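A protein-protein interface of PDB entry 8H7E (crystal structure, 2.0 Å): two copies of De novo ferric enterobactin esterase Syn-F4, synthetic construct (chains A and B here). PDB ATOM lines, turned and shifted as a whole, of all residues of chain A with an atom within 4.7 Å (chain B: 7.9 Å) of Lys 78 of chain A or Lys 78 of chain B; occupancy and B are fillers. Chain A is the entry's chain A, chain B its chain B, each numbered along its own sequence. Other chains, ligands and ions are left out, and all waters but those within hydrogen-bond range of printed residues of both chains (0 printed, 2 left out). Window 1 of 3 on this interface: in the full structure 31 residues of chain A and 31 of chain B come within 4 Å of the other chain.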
ATOM      1  N   TRP A  23      17.363  -6.746  -6.869  1.00  0.00           N
ATOM      2  CA  TRP A  23      17.058  -7.956  -7.643  1.00  0.00           C
ATOM      3  C   TRP A  23      17.474  -7.741  -9.115  1.00  0.00           C
ATOM      4  O   TRP A  23      18.164  -8.590  -9.705  1.00  0.00           O
ATOM      5  CB  TRP A  23      15.565  -8.344  -7.543  1.00  0.00           C
ATOM      6  CG  TRP A  23      15.171  -9.092  -6.245  1.00  0.00           C
ATOM      7  CD1 TRP A  23      15.976  -9.946  -5.503  1.00  0.00           C
ATOM      8  CD2 TRP A  23      13.898  -9.062  -5.563  1.00  0.00           C
ATOM      9  NE1 TRP A  23      15.282 -10.412  -4.406  1.00  0.00           N
ATOM     10  CE2 TRP A  23      14.002  -9.920  -4.443  1.00  0.00           C
ATOM     11  CE3 TRP A  23      12.675  -8.416  -5.809  1.00  0.00           C
ATOM     12  CZ2 TRP A  23      12.937 -10.142  -3.576  1.00  0.00           C
ATOM     13  CZ3 TRP A  23      11.615  -8.632  -4.943  1.00  0.00           C
ATOM     14  CH2 TRP A  23      11.751  -9.484  -3.841  1.00  0.00           C
ATOM     15  N   GLU A  26      21.441  -7.660  -9.164  1.00  0.00           N
ATOM     16  CA  GLU A  26      21.864  -9.026  -8.897  1.00  0.00           C
ATOM     17  C   GLU A  26      21.692  -9.959 -10.135  1.00  0.00           C
ATOM     18  O   GLU A  26      22.610 -10.710 -10.502  1.00  0.00           O
ATOM     19  CB  GLU A  26      21.026  -9.512  -7.718  1.00  0.00           C
ATOM     20  CG  GLU A  26      20.997 -10.970  -7.424  1.00  0.00           C
ATOM     21  CD  GLU A  26      20.426 -11.220  -6.034  1.00  0.00           C
ATOM     22  OE1 GLU A  26      19.307 -10.781  -5.687  1.00  0.00           O
ATOM     23  OE2 GLU A  26      21.124 -11.829  -5.248  1.00  0.00           O
ATOM     24  N   HIS A  74      20.393 -22.367 -10.734  1.00  0.00           N
ATOM     25  CA  HIS A  74      20.242 -21.339  -9.728  1.00  0.00           C
ATOM     26  C   HIS A  74      19.488 -20.068 -10.170  1.00  0.00           C
ATOM     27  O   HIS A  74      18.583 -19.600  -9.481  1.00  0.00           O
ATOM     28  CB  HIS A  74      21.622 -21.000  -9.179  1.00  0.00           C
ATOM     29  CG  HIS A  74      21.604 -19.895  -8.183  1.00  0.00           C
ATOM     30  ND1 HIS A  74      21.063 -20.035  -6.929  1.00  0.00           N
ATOM     31  CD2 HIS A  74      22.014 -18.612  -8.277  1.00  0.00           C
ATOM     32  CE1 HIS A  74      21.145 -18.887  -6.289  1.00  0.00           C
ATOM     33  NE2 HIS A  74      21.723 -18.008  -7.085  1.00  0.00           N
ATOM     34  N   LEU A  75      19.882 -19.512 -11.312  1.00  0.00           N
ATOM     35  CA  LEU A  75      19.284 -18.308 -11.871  1.00  0.00           C
ATOM     36  C   LEU A  75      17.816 -18.502 -12.320  1.00  0.00           C
ATOM     37  O   LEU A  75      16.973 -17.615 -12.103  1.00  0.00           O
ATOM     38  CB  LEU A  75      20.147 -17.829 -13.039  1.00  0.00           C
ATOM     39  CG  LEU A  75      21.535 -17.306 -12.603  1.00  0.00           C
ATOM     40  CD1 LEU A  75      22.385 -16.977 -13.804  1.00  0.00           C
ATOM     41  CD2 LEU A  75      21.425 -16.082 -11.698  1.00  0.00           C
ATOM     42  N   GLN A  76      17.502 -19.644 -12.943  1.00  0.00           N
ATOM     43  CA  GLN A  76      16.096 -19.993 -13.189  1.00  0.00           C
ATOM     44  C   GLN A  76      15.224 -20.060 -11.896  1.00  0.00           C
ATOM     45  O   GLN A  76      14.173 -19.398 -11.808  1.00  0.00           O
ATOM     46  CB  GLN A  76      15.986 -21.317 -13.961  1.00  0.00           C
ATOM     47  CG  GLN A  76      16.418 -21.205 -15.412  1.00  0.00           C
ATOM     48  CD  GLN A  76      16.325 -22.552 -16.114  1.00  0.00           C
ATOM     49  OE1 GLN A  76      15.221 -23.126 -16.256  1.00  0.00           O
ATOM     50  NE2 GLN A  76      17.477 -23.112 -16.476  1.00  0.00           N
ATOM     51  N   ARG A  77      15.722 -20.759 -10.879  1.00  0.00           N
ATOM     52  CA  ARG A  77      15.037 -20.872  -9.594  1.00  0.00           C
ATOM     53  C   ARG A  77      14.913 -19.495  -8.946  1.00  0.00           C
ATOM     54  O   ARG A  77      13.862 -19.147  -8.367  1.00  0.00           O
ATOM     55  CB  ARG A  77      15.812 -21.780  -8.632  1.00  0.00           C
ATOM     56  CG  ARG A  77      16.127 -23.181  -9.173  1.00  0.00           C
ATOM     57  CD  ARG A  77      15.332 -24.269  -8.519  1.00  0.00           C
ATOM     58  NE  ARG A  77      15.492 -24.242  -7.069  1.00  0.00           N
ATOM     59  CZ  ARG A  77      14.580 -24.683  -6.198  1.00  0.00           C
ATOM     60  NH1 ARG A  77      13.424 -25.231  -6.622  1.00  0.00           N
ATOM     61  NH2 ARG A  77      14.825 -24.585  -4.891  1.00  0.00           N
ATOM     62  N   LYS A  78      16.000 -18.710  -9.033  1.00  0.00           N
ATOM     63  CA  LYS A  78      15.995 -17.396  -8.454  1.00  0.00           C
ATOM     64  C   LYS A  78      14.902 -16.556  -9.111  1.00  0.00           C
ATOM     65  O   LYS A  78      14.156 -15.910  -8.409  1.00  0.00           O
ATOM     66  CB  LYS A  78      17.371 -16.763  -8.565  1.00  0.00           C
ATOM     67  CG  LYS A  78      17.521 -15.369  -7.972  1.00  0.00           C
ATOM     68  CD  LYS A  78      17.607 -15.352  -6.445  1.00  0.00           C
ATOM     69  CE  LYS A  78      18.339 -14.091  -5.979  1.00  0.00           C
ATOM     70  NZ  LYS A  78      17.983 -13.617  -4.605  1.00  0.00           N
ATOM     71  N   ASP A  79      14.763 -16.590 -10.438  1.00  0.00           N
ATOM     72  CA  ASP A  79      13.708 -15.790 -11.098  1.00  0.00           C
ATOM     73  C   ASP A  79      12.341 -16.172 -10.570  1.00  0.00           C
ATOM     74  O   ASP A  79      11.488 -15.321 -10.393  1.00  0.00           O
ATOM     75  CB  ASP A  79      13.689 -15.963 -12.629  1.00  0.00           C
ATOM     76  CG  ASP A  79      14.732 -15.126 -13.343  1.00  0.00           C
ATOM     77  OD1 ASP A  79      15.238 -14.120 -12.842  1.00  0.00           O
ATOM     78  OD2 ASP A  79      15.031 -15.450 -14.495  1.00  0.00           O
ATOM     79  N   ASP A  80      12.132 -17.474 -10.374  1.00  0.00           N
ATOM     80  CA  ASP A  80      10.875 -17.991  -9.847  1.00  0.00           C
ATOM     81  C   ASP A  80      10.555 -17.512  -8.436  1.00  0.00           C
ATOM     82  O   ASP A  80       9.424 -17.069  -8.183  1.00  0.00           O
ATOM     83  CB  ASP A  80      10.863 -19.533  -9.915  1.00  0.00           C
ATOM     84  CG  ASP A  80      10.780 -20.055 -11.350  1.00  0.00           C
ATOM     85  OD1 ASP A  80      10.297 -19.309 -12.228  1.00  0.00           O
ATOM     86  OD2 ASP A  80      11.179 -21.209 -11.615  1.00  0.00           O
ATOM     87  N   THR A  81      11.556 -17.582  -7.545  1.00  0.00           N
ATOM     88  CA  THR A  81      11.416 -17.172  -6.159  1.00  0.00           C
ATOM     89  C   THR A  81      11.191 -15.662  -6.046  1.00  0.00           C
ATOM     90  O   THR A  81      10.359 -15.210  -5.272  1.00  0.00           O
ATOM     91  CB  THR A  81      12.661 -17.580  -5.320  1.00  0.00           C
ATOM     92  OG1 THR A  81      12.919 -18.980  -5.515  1.00  0.00           O
ATOM     93  CG2 THR A  81      12.440 -17.337  -3.843  1.00  0.00           C
ATOM     94  N   VAL A  82      11.917 -14.903  -6.850  1.00  0.00           N
ATOM     95  CA  VAL A  82      11.744 -13.469  -6.896  1.00  0.00           C
ATOM     96  C   VAL A  82      10.337 -13.115  -7.379  1.00  0.00           C
ATOM     97  O   VAL A  82       9.673 -12.266  -6.786  1.00  0.00           O
ATOM     98  CB  VAL A  82      12.796 -12.814  -7.787  1.00  0.00           C
ATOM     99  CG1 VAL A  82      12.478 -11.327  -7.960  1.00  0.00           C
ATOM    100  CG2 VAL A  82      14.189 -13.006  -7.193  1.00  0.00           C
ATOM    101  N   LEU B  19      12.730 -14.254   3.307  1.00  0.00           N
ATOM    102  CA  LEU B  19      13.842 -13.492   2.680  1.00  0.00           C
ATOM    103  C   LEU B  19      15.181 -13.856   3.268  1.00  0.00           C
ATOM    104  O   LEU B  19      16.165 -14.009   2.534  1.00  0.00           O
ATOM    105  CB  LEU B  19      13.656 -11.983   2.787  1.00  0.00           C
ATOM    106  CG  LEU B  19      12.598 -11.340   1.891  1.00  0.00           C
ATOM    107  CD1 LEU B  19      12.346  -9.906   2.374  1.00  0.00           C
ATOM    108  CD2 LEU B  19      13.037 -11.392   0.431  1.00  0.00           C
ATOM    109  N   ASN B  22      16.140 -17.601   2.363  1.00  0.00           N
ATOM    110  CA  ASN B  22      16.601 -17.725   0.995  1.00  0.00           C
ATOM    111  C   ASN B  22      18.020 -17.173   0.842  1.00  0.00           C
ATOM    112  O   ASN B  22      18.814 -17.742   0.118  1.00  0.00           O
ATOM    113  CB  ASN B  22      15.666 -17.038  -0.003  1.00  0.00           C
ATOM    114  CG  ASN B  22      14.289 -17.676  -0.080  1.00  0.00           C
ATOM    115  OD1 ASN B  22      13.291 -16.957  -0.198  1.00  0.00           O
ATOM    116  ND2 ASN B  22      14.217 -19.009  -0.052  1.00  0.00           N
ATOM    117  N   TRP B  23      18.358 -16.075   1.515  1.00  0.00           N
ATOM    118  CA  TRP B  23      19.747 -15.585   1.452  1.00  0.00           C
ATOM    119  C   TRP B  23      20.707 -16.575   2.124  1.00  0.00           C
ATOM    120  O   TRP B  23      21.731 -16.887   1.557  1.00  0.00           O
ATOM    121  CB  TRP B  23      19.906 -14.226   2.081  1.00  0.00           C
ATOM    122  CG  TRP B  23      21.347 -13.819   2.162  1.00  0.00           C
ATOM    123  CD1 TRP B  23      22.028 -13.489   3.292  1.00  0.00           C
ATOM    124  CD2 TRP B  23      22.308 -13.783   1.088  1.00  0.00           C
ATOM    125  NE1 TRP B  23      23.332 -13.189   2.983  1.00  0.00           N
ATOM    126  CE2 TRP B  23      23.535 -13.365   1.644  1.00  0.00           C
ATOM    127  CE3 TRP B  23      22.245 -14.035  -0.286  1.00  0.00           C
ATOM    128  CZ2 TRP B  23      24.689 -13.202   0.882  1.00  0.00           C
ATOM    129  CZ3 TRP B  23      23.403 -13.871  -1.049  1.00  0.00           C
ATOM    130  CH2 TRP B  23      24.603 -13.448  -0.461  1.00  0.00           C
ATOM    131  N   GLU B  26      21.121 -19.165  -0.606  1.00  0.00           N
ATOM    132  CA  GLU B  26      21.838 -18.667  -1.761  1.00  0.00           C
ATOM    133  C   GLU B  26      23.312 -18.435  -1.408  1.00  0.00           C
ATOM    134  O   GLU B  26      24.178 -18.794  -2.200  1.00  0.00           O
ATOM    135  CB  GLU B  26      21.191 -17.395  -2.326  1.00  0.00           C
ATOM    136  CG  GLU B  26      21.991 -16.804  -3.470  1.00  0.00           C
ATOM    137  CD  GLU B  26      21.255 -15.731  -4.255  1.00  0.00           C
ATOM    138  OE1 GLU B  26      20.375 -15.043  -3.667  1.00  0.00           O
ATOM    139  OE2 GLU B  26      21.599 -15.578  -5.462  1.00  0.00           O
ATOM    140  N   ARG B  27      23.577 -17.853  -0.233  1.00  0.00           N
ATOM    141  CA  ARG B  27      24.949 -17.613   0.221  1.00  0.00           C
ATOM    142  C   ARG B  27      25.782 -18.897   0.215  1.00  0.00           C
ATOM    143  O   ARG B  27      26.874 -18.921  -0.340  1.00  0.00           O
ATOM    144  CB  ARG B  27      24.962 -16.989   1.616  1.00  0.00           C
ATOM    145  CG  ARG B  27      26.350 -16.549   2.053  1.00  0.00           C
ATOM    146  CD  ARG B  27      26.390 -15.999   3.472  1.00  0.00           C
ATOM    147  NE  ARG B  27      27.567 -15.154   3.679  1.00  0.00           N
ATOM    148  CZ  ARG B  27      28.632 -15.480   4.405  1.00  0.00           C
ATOM    149  NH1 ARG B  27      28.697 -16.648   5.039  1.00  0.00           N
ATOM    150  NH2 ARG B  27      29.640 -14.624   4.502  1.00  0.00           N
ATOM    151  N   LEU B  30      26.295 -20.174  -3.447  1.00  0.00           N
ATOM    152  CA  LEU B  30      27.294 -19.361  -4.148  1.00  0.00           C
ATOM    153  C   LEU B  30      28.699 -19.481  -3.557  1.00  0.00           C
ATOM    154  O   LEU B  30      29.679 -19.405  -4.307  1.00  0.00           O
ATOM    155  CB  LEU B  30      26.863 -17.911  -4.173  1.00  0.00           C
ATOM    156  CG  LEU B  30      25.684 -17.528  -5.084  1.00  0.00           C
ATOM    157  CD1 LEU B  30      25.405 -16.028  -4.945  1.00  0.00           C
ATOM    158  CD2 LEU B  30      25.932 -17.878  -6.535  1.00  0.00           C
ATOM    159  N   LEU B  71      32.655 -13.161  -8.135  1.00  0.00           N
ATOM    160  CA  LEU B  71      31.692 -13.815  -7.279  1.00  0.00           C
ATOM    161  C   LEU B  71      31.922 -13.511  -5.794  1.00  0.00           C
ATOM    162  O   LEU B  71      30.966 -13.292  -5.035  1.00  0.00           O
ATOM    163  CB  LEU B  71      31.727 -15.318  -7.553  1.00  0.00           C
ATOM    164  CG  LEU B  71      30.631 -16.132  -6.880  1.00  0.00           C
ATOM    165  CD1 LEU B  71      29.268 -15.515  -7.203  1.00  0.00           C
ATOM    166  CD2 LEU B  71      30.691 -17.574  -7.347  1.00  0.00           C
ATOM    167  N   ASP B  72      33.186 -13.465  -5.385  1.00  0.00           N
ATOM    168  CA  ASP B  72      33.524 -13.101  -4.012  1.00  0.00           C
ATOM    169  C   ASP B  72      33.054 -11.674  -3.694  1.00  0.00           C
ATOM    170  O   ASP B  72      32.447 -11.430  -2.643  1.00  0.00           O
ATOM    171  CB  ASP B  72      35.034 -13.238  -3.784  1.00  0.00           C
ATOM    172  CG  ASP B  72      35.425 -13.114  -2.320  1.00  0.00           C
ATOM    173  OD1 ASP B  72      34.766 -13.708  -1.447  1.00  0.00           O
ATOM    174  OD2 ASP B  72      36.411 -12.425  -2.042  1.00  0.00           O
ATOM    175  N   ASN B  73      33.323 -10.757  -4.627  1.00  0.00           N
ATOM    176  CA  ASN B  73      32.915  -9.341  -4.523  1.00  0.00           C
ATOM    177  C   ASN B  73      31.410  -9.240  -4.304  1.00  0.00           C
ATOM    178  O   ASN B  73      30.930  -8.648  -3.346  1.00  0.00           O
ATOM    179  CB  ASN B  73      33.330  -8.588  -5.799  1.00  0.00           C
ATOM    180  CG  ASN B  73      32.899  -7.129  -5.795  1.00  0.00           C
ATOM    181  OD1 ASN B  73      33.544  -6.312  -5.175  1.00  0.00           O
ATOM    182  ND2 ASN B  73      31.823  -6.803  -6.503  1.00  0.00           N
ATOM    183  N   HIS B  74      30.690  -9.896  -5.191  1.00  0.00           N
ATOM    184  CA  HIS B  74      29.265  -9.979  -5.138  1.00  0.00           C
ATOM    185  C   HIS B  74      28.724 -10.493  -3.806  1.00  0.00           C
ATOM    186  O   HIS B  74      27.776  -9.929  -3.283  1.00  0.00           O
ATOM    187  CB  HIS B  74      28.797 -10.879  -6.275  1.00  0.00           C
ATOM    188  CG  HIS B  74      27.334 -11.152  -6.245  1.00  0.00           C
ATOM    189  ND1 HIS B  74      26.394 -10.170  -6.479  1.00  0.00           N
ATOM    190  CD2 HIS B  74      26.647 -12.278  -5.973  1.00  0.00           C
ATOM    191  CE1 HIS B  74      25.189 -10.691  -6.382  1.00  0.00           C
ATOM    192  NE2 HIS B  74      25.316 -11.964  -6.068  1.00  0.00           N
ATOM    193  N   LEU B  75      29.318 -11.566  -3.275  1.00  0.00           N
ATOM    194  CA  LEU B  75      28.848 -12.169  -2.020  1.00  0.00           C
ATOM    195  C   LEU B  75      29.060 -11.240  -0.824  1.00  0.00           C
ATOM    196  O   LEU B  75      28.159 -11.077  -0.006  1.00  0.00           O
ATOM    197  CB  LEU B  75      29.532 -13.511  -1.766  1.00  0.00           C
ATOM    198  CG  LEU B  75      29.100 -14.673  -2.667  1.00  0.00           C
ATOM    199  CD1 LEU B  75      29.751 -15.964  -2.210  1.00  0.00           C
ATOM    200  CD2 LEU B  75      27.589 -14.820  -2.706  1.00  0.00           C
ATOM    201  N   GLN B  76      30.247 -10.647  -0.745  1.00  0.00           N
ATOM    202  CA  GLN B  76      30.564  -9.615   0.257  1.00  0.00           C
ATOM    203  C   GLN B  76      29.593  -8.443   0.156  1.00  0.00           C
ATOM    204  O   GLN B  76      29.008  -8.016   1.148  1.00  0.00           O
ATOM    205  CB  GLN B  76      31.997  -9.101   0.056  1.00  0.00           C
ATOM    206  CG  GLN B  76      33.062 -10.145   0.349  1.00  0.00           C
ATOM    207  CD  GLN B  76      34.470  -9.607   0.240  1.00  0.00           C
ATOM    208  OE1 GLN B  76      35.144  -9.789  -0.771  1.00  0.00           O
ATOM    209  NE2 GLN B  76      34.919  -8.927   1.280  1.00  0.00           N
ATOM    210  N   ARG B  77      29.391  -7.955  -1.062  1.00  0.00           N
ATOM    211  CA  ARG B  77      28.494  -6.816  -1.266  1.00  0.00           C
ATOM    212  C   ARG B  77      27.045  -7.165  -0.982  1.00  0.00           C
ATOM    213  O   ARG B  77      26.346  -6.375  -0.353  1.00  0.00           O
ATOM    214  CB  ARG B  77      28.672  -6.187  -2.650  1.00  0.00           C
ATOM    215  CG  ARG B  77      29.765  -5.124  -2.638  1.00  0.00           C
ATOM    216  CD  ARG B  77      29.763  -4.247  -3.870  1.00  0.00           C
ATOM    217  NE  ARG B  77      28.465  -3.635  -4.188  1.00  0.00           N
ATOM    218  CZ  ARG B  77      28.091  -2.384  -3.916  1.00  0.00           C
ATOM    219  NH1 ARG B  77      28.900  -1.518  -3.302  1.00  0.00           N
ATOM    220  NH2 ARG B  77      26.878  -1.973  -4.297  1.00  0.00           N
ATOM    221  N   LYS B  78      26.592  -8.350  -1.388  1.00  0.00           N
ATOM    222  CA  LYS B  78      25.227  -8.739  -1.060  1.00  0.00           C
ATOM    223  C   LYS B  78      25.054  -8.960   0.434  1.00  0.00           C
ATOM    224  O   LYS B  78      24.031  -8.574   1.007  1.00  0.00           O
ATOM    225  CB  LYS B  78      24.760  -9.978  -1.851  1.00  0.00           C
ATOM    226  CG  LYS B  78      23.280 -10.196  -1.622  1.00  0.00           C
ATOM    227  CD  LYS B  78      22.517 -10.928  -2.703  1.00  0.00           C
ATOM    228  CE  LYS B  78      21.099 -11.141  -2.187  1.00  0.00           C
ATOM    229  NZ  LYS B  78      20.383 -12.157  -2.969  1.00  0.00           N
ATOM    230  N   ASP B  79      26.048  -9.565   1.070  1.00  0.00           N
ATOM    231  CA  ASP B  79      25.974  -9.815   2.512  1.00  0.00           C
ATOM    232  C   ASP B  79      25.704  -8.503   3.276  1.00  0.00           C
ATOM    233  O   ASP B  79      24.810  -8.448   4.117  1.00  0.00           O
ATOM    234  CB  ASP B  79      27.247 -10.536   2.999  1.00  0.00           C
ATOM    235  CG  ASP B  79      27.018 -11.391   4.258  1.00  0.00           C
ATOM    236  OD1 ASP B  79      26.014 -12.152   4.381  1.00  0.00           O
ATOM    237  OD2 ASP B  79      27.876 -11.284   5.149  1.00  0.00           O
ATOM    238  N   ASP B  80      26.415  -7.437   2.901  1.00  0.00           N
ATOM    239  CA  ASP B  80      26.225  -6.113   3.499  1.00  0.00           C
ATOM    240  C   ASP B  80      24.833  -5.549   3.204  1.00  0.00           C
ATOM    241  O   ASP B  80      24.170  -5.002   4.095  1.00  0.00           O
ATOM    242  CB  ASP B  80      27.311  -5.135   3.013  1.00  0.00           C
ATOM    243  CG  ASP B  80      28.726  -5.501   3.512  1.00  0.00           C
ATOM    244  OD1 ASP B  80      28.843  -6.068   4.610  1.00  0.00           O
ATOM    245  OD2 ASP B  80      29.724  -5.216   2.797  1.00  0.00           O
ATOM    246  N   THR B  81      24.373  -5.729   1.971  1.00  0.00           N
ATOM    247  CA  THR B  81      23.056  -5.233   1.574  1.00  0.00           C
ATOM    248  C   THR B  81      21.969  -5.961   2.344  1.00  0.00           C
ATOM    249  O   THR B  81      21.094  -5.318   2.908  1.00  0.00           O
ATOM    250  CB  THR B  81      22.835  -5.371   0.043  1.00  0.00           C
ATOM    251  OG1 THR B  81      23.910  -4.730  -0.656  1.00  0.00           O
ATOM    252  CG2 THR B  81      21.468  -4.761  -0.398  1.00  0.00           C
ATOM    253  N   VAL B  82      22.069  -7.295   2.424  1.00  0.00           N
ATOM    254  CA  VAL B  82      21.125  -8.106   3.208  1.00  0.00           C
ATOM    255  C   VAL B  82      21.108  -7.720   4.705  1.00  0.00           C
ATOM    256  O   VAL B  82      20.029  -7.491   5.294  1.00  0.00           O
ATOM    257  CB  VAL B  82      21.407  -9.631   3.038  1.00  0.00           C
ATOM    258  CG1 VAL B  82      20.492 -10.476   3.933  1.00  0.00           C
ATOM    259  CG2 VAL B  82      21.194 -10.062   1.589  1.00  0.00           C
ATOM    260  N   HIS B  83      22.295  -7.610   5.312  1.00  0.00           N
ATOM    261  CA  HIS B  83      22.413  -7.165   6.714  1.00  0.00           C
ATOM    262  C   HIS B  83      21.566  -5.895   6.944  1.00  0.00           C
ATOM    263  O   HIS B  83      20.688  -5.867   7.804  1.00  0.00           O
ATOM    264  CB  HIS B  83      23.894  -6.948   7.084  1.00  0.00           C
ATOM    265  CG  HIS B  83      24.122  -6.209   8.375  1.00  0.00           C
ATOM    266  ND1 HIS B  83      24.282  -6.850   9.588  1.00  0.00           N
ATOM    267  CD2 HIS B  83      24.264  -4.885   8.633  1.00  0.00           C
ATOM    268  CE1 HIS B  83      24.482  -5.952  10.537  1.00  0.00           C
ATOM    269  NE2 HIS B  83      24.485  -4.754   9.983  1.00  0.00           N
ATOM    270  N   HIS B  84      21.789  -4.896   6.101  1.00  0.00           N
ATOM    271  CA  HIS B  84      21.090  -3.624   6.174  1.00  0.00           C
ATOM    272  C   HIS B  84      19.558  -3.729   5.979  1.00  0.00           C
ATOM    273  O   HIS B  84      18.803  -3.161   6.754  1.00  0.00           O
ATOM    274  CB  HIS B  84      21.736  -2.637   5.185  1.00  0.00           C
ATOM    275  CG  HIS B  84      21.010  -1.341   5.085  1.00  0.00           C
ATOM    276  ND1 HIS B  84      20.359  -0.948   3.936  1.00  0.00           N
ATOM    277  CD2 HIS B  84      20.765  -0.385   6.010  1.00  0.00           C
ATOM    278  CE1 HIS B  84      19.779   0.221   4.151  1.00  0.00           C
ATOM    279  NE2 HIS B  84      19.990   0.571   5.409  1.00  0.00           N
ATOM    280  N   ARG B  85      19.088  -4.458   4.971  1.00  0.00           N
ATOM    281  CA  ARG B  85      17.619  -4.626   4.782  1.00  0.00           C
ATOM    282  C   ARG B  85      16.931  -5.406   5.903  1.00  0.00           C
ATOM    283  O   ARG B  85      15.780  -5.117   6.227  1.00  0.00           O
ATOM    284  CB  ARG B  85      17.295  -5.293   3.444  1.00  0.00           C
ATOM    285  CG  ARG B  85      17.287  -6.806   3.483  1.00  0.00           C
ATOM    286  CD  ARG B  85      17.114  -7.442   2.122  1.00  0.00           C
ATOM    287  NE  ARG B  85      17.089  -8.910   2.266  1.00  0.00           N
ATOM    288  CZ  ARG B  85      17.375  -9.784   1.298  1.00  0.00           C
ATOM    289  NH1 ARG B  85      17.725  -9.370   0.074  1.00  0.00           N
ATOM    290  NH2 ARG B  85      17.341 -11.088   1.562  1.00  0.00           N
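A ring nitrogen (NE2) of His 74 of chain A lies within hydrogen-bond range of the side-chain carboxylate (OE2) of Glu 26 of chain B (2.9 Å). The side-chain carboxylate (OE2) of Glu 26 of chain A is in salt-bridge range of the side-chain amino group (NZ) of Lys 78 of chain B (2.4 Å). The side-chain amino group of Lys 78 of chain A is in salt-bridge range of the side-chain carboxylate of Glu 26 of chain B (2.9 Å). NZ of Lys 78 of chain B sits close to NZ of Lys 78 of chain A.
OE1 of Glu 26 of chain A is in salt-bridge range of NZ of Lys 78 of chain A. The side-chain amino group (NZ) of Lys 78 of chain B lies within salt-bridge range of the side-chain carboxylate (OE1) of Glu 26 of chain B. The side-chain hydroxyl of Thr 81 of chain A is in hydrogen-bond range of the backbone carbonyl oxygen of Arg 77 of chain A (3.0 Å).
Among the printed residues, pairs that only touch across the chains: Glu 26 of chain A with Glu 26 of chain B and Thr 81 of chain A with Asn 22 of chain B.
Of chain A, only Glu 26 (2.4 Å) and Lys 78 (3.3 Å) come within 4 Å of Lys 78 of chain B. Of the printed residues of chain A, Asn 22 of chain B touches Thr 81. Of the printed residues of chain B, Thr 81 of chain A touches Asn 22. Printed residues of chain B within 4 Å of His 74 of chain A: Glu 26. Asp 72 of chain B touches none of the printed residues of chain A. The nearest residue of chain B that does not touch Lys 78 of chain A is Trp 23 of chain B (6.1 Å). The nearest printed residue of chain A that does not touch Glu 26 of chain B is Leu 75 of chain A (6.3 Å).
Hydrophobic or aromatic side chains of chain A that line the printed part of chain B: His 74. Of the 21 printed residues of chain B, 3 touch a printed residue of chain A. Printed residues of chain B that touch a printed residue of chain A: Asn 22, Glu 26 and Lys 78. Among the printed residues, 6 pairs touch across the chains. Among the printed residues, Asp or Glu carboxylates within 4 Å of a Lys or Arg side-chain nitrogen of the other chain: Glu 26 of chain A with Lys 78 of chain B (2.4 Å) and Lys 78 of chain A with Glu 26 of chain B (2.9 Å).
Glu 26 of chain A touches its own counterpart, Glu 26 of chain B. Glu 26 of chain A touches Lys 78 of chain B, and with the chains exchanged Lys 78 of chain A touches Glu 26 of chain B. His 74 of chain A touches Glu 26 of chain B, but with the chains exchanged Glu 26 of chain A does not touch His 74 of chain B (4.3 Å). Lys 78 of chain B touches its own counterpart, Lys 78 of chain A. 11 positions are printed for both chains. Of the 6 pairs that touch across the chains among the printed residues, 4 have their exchanged pair printed and touching as well.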
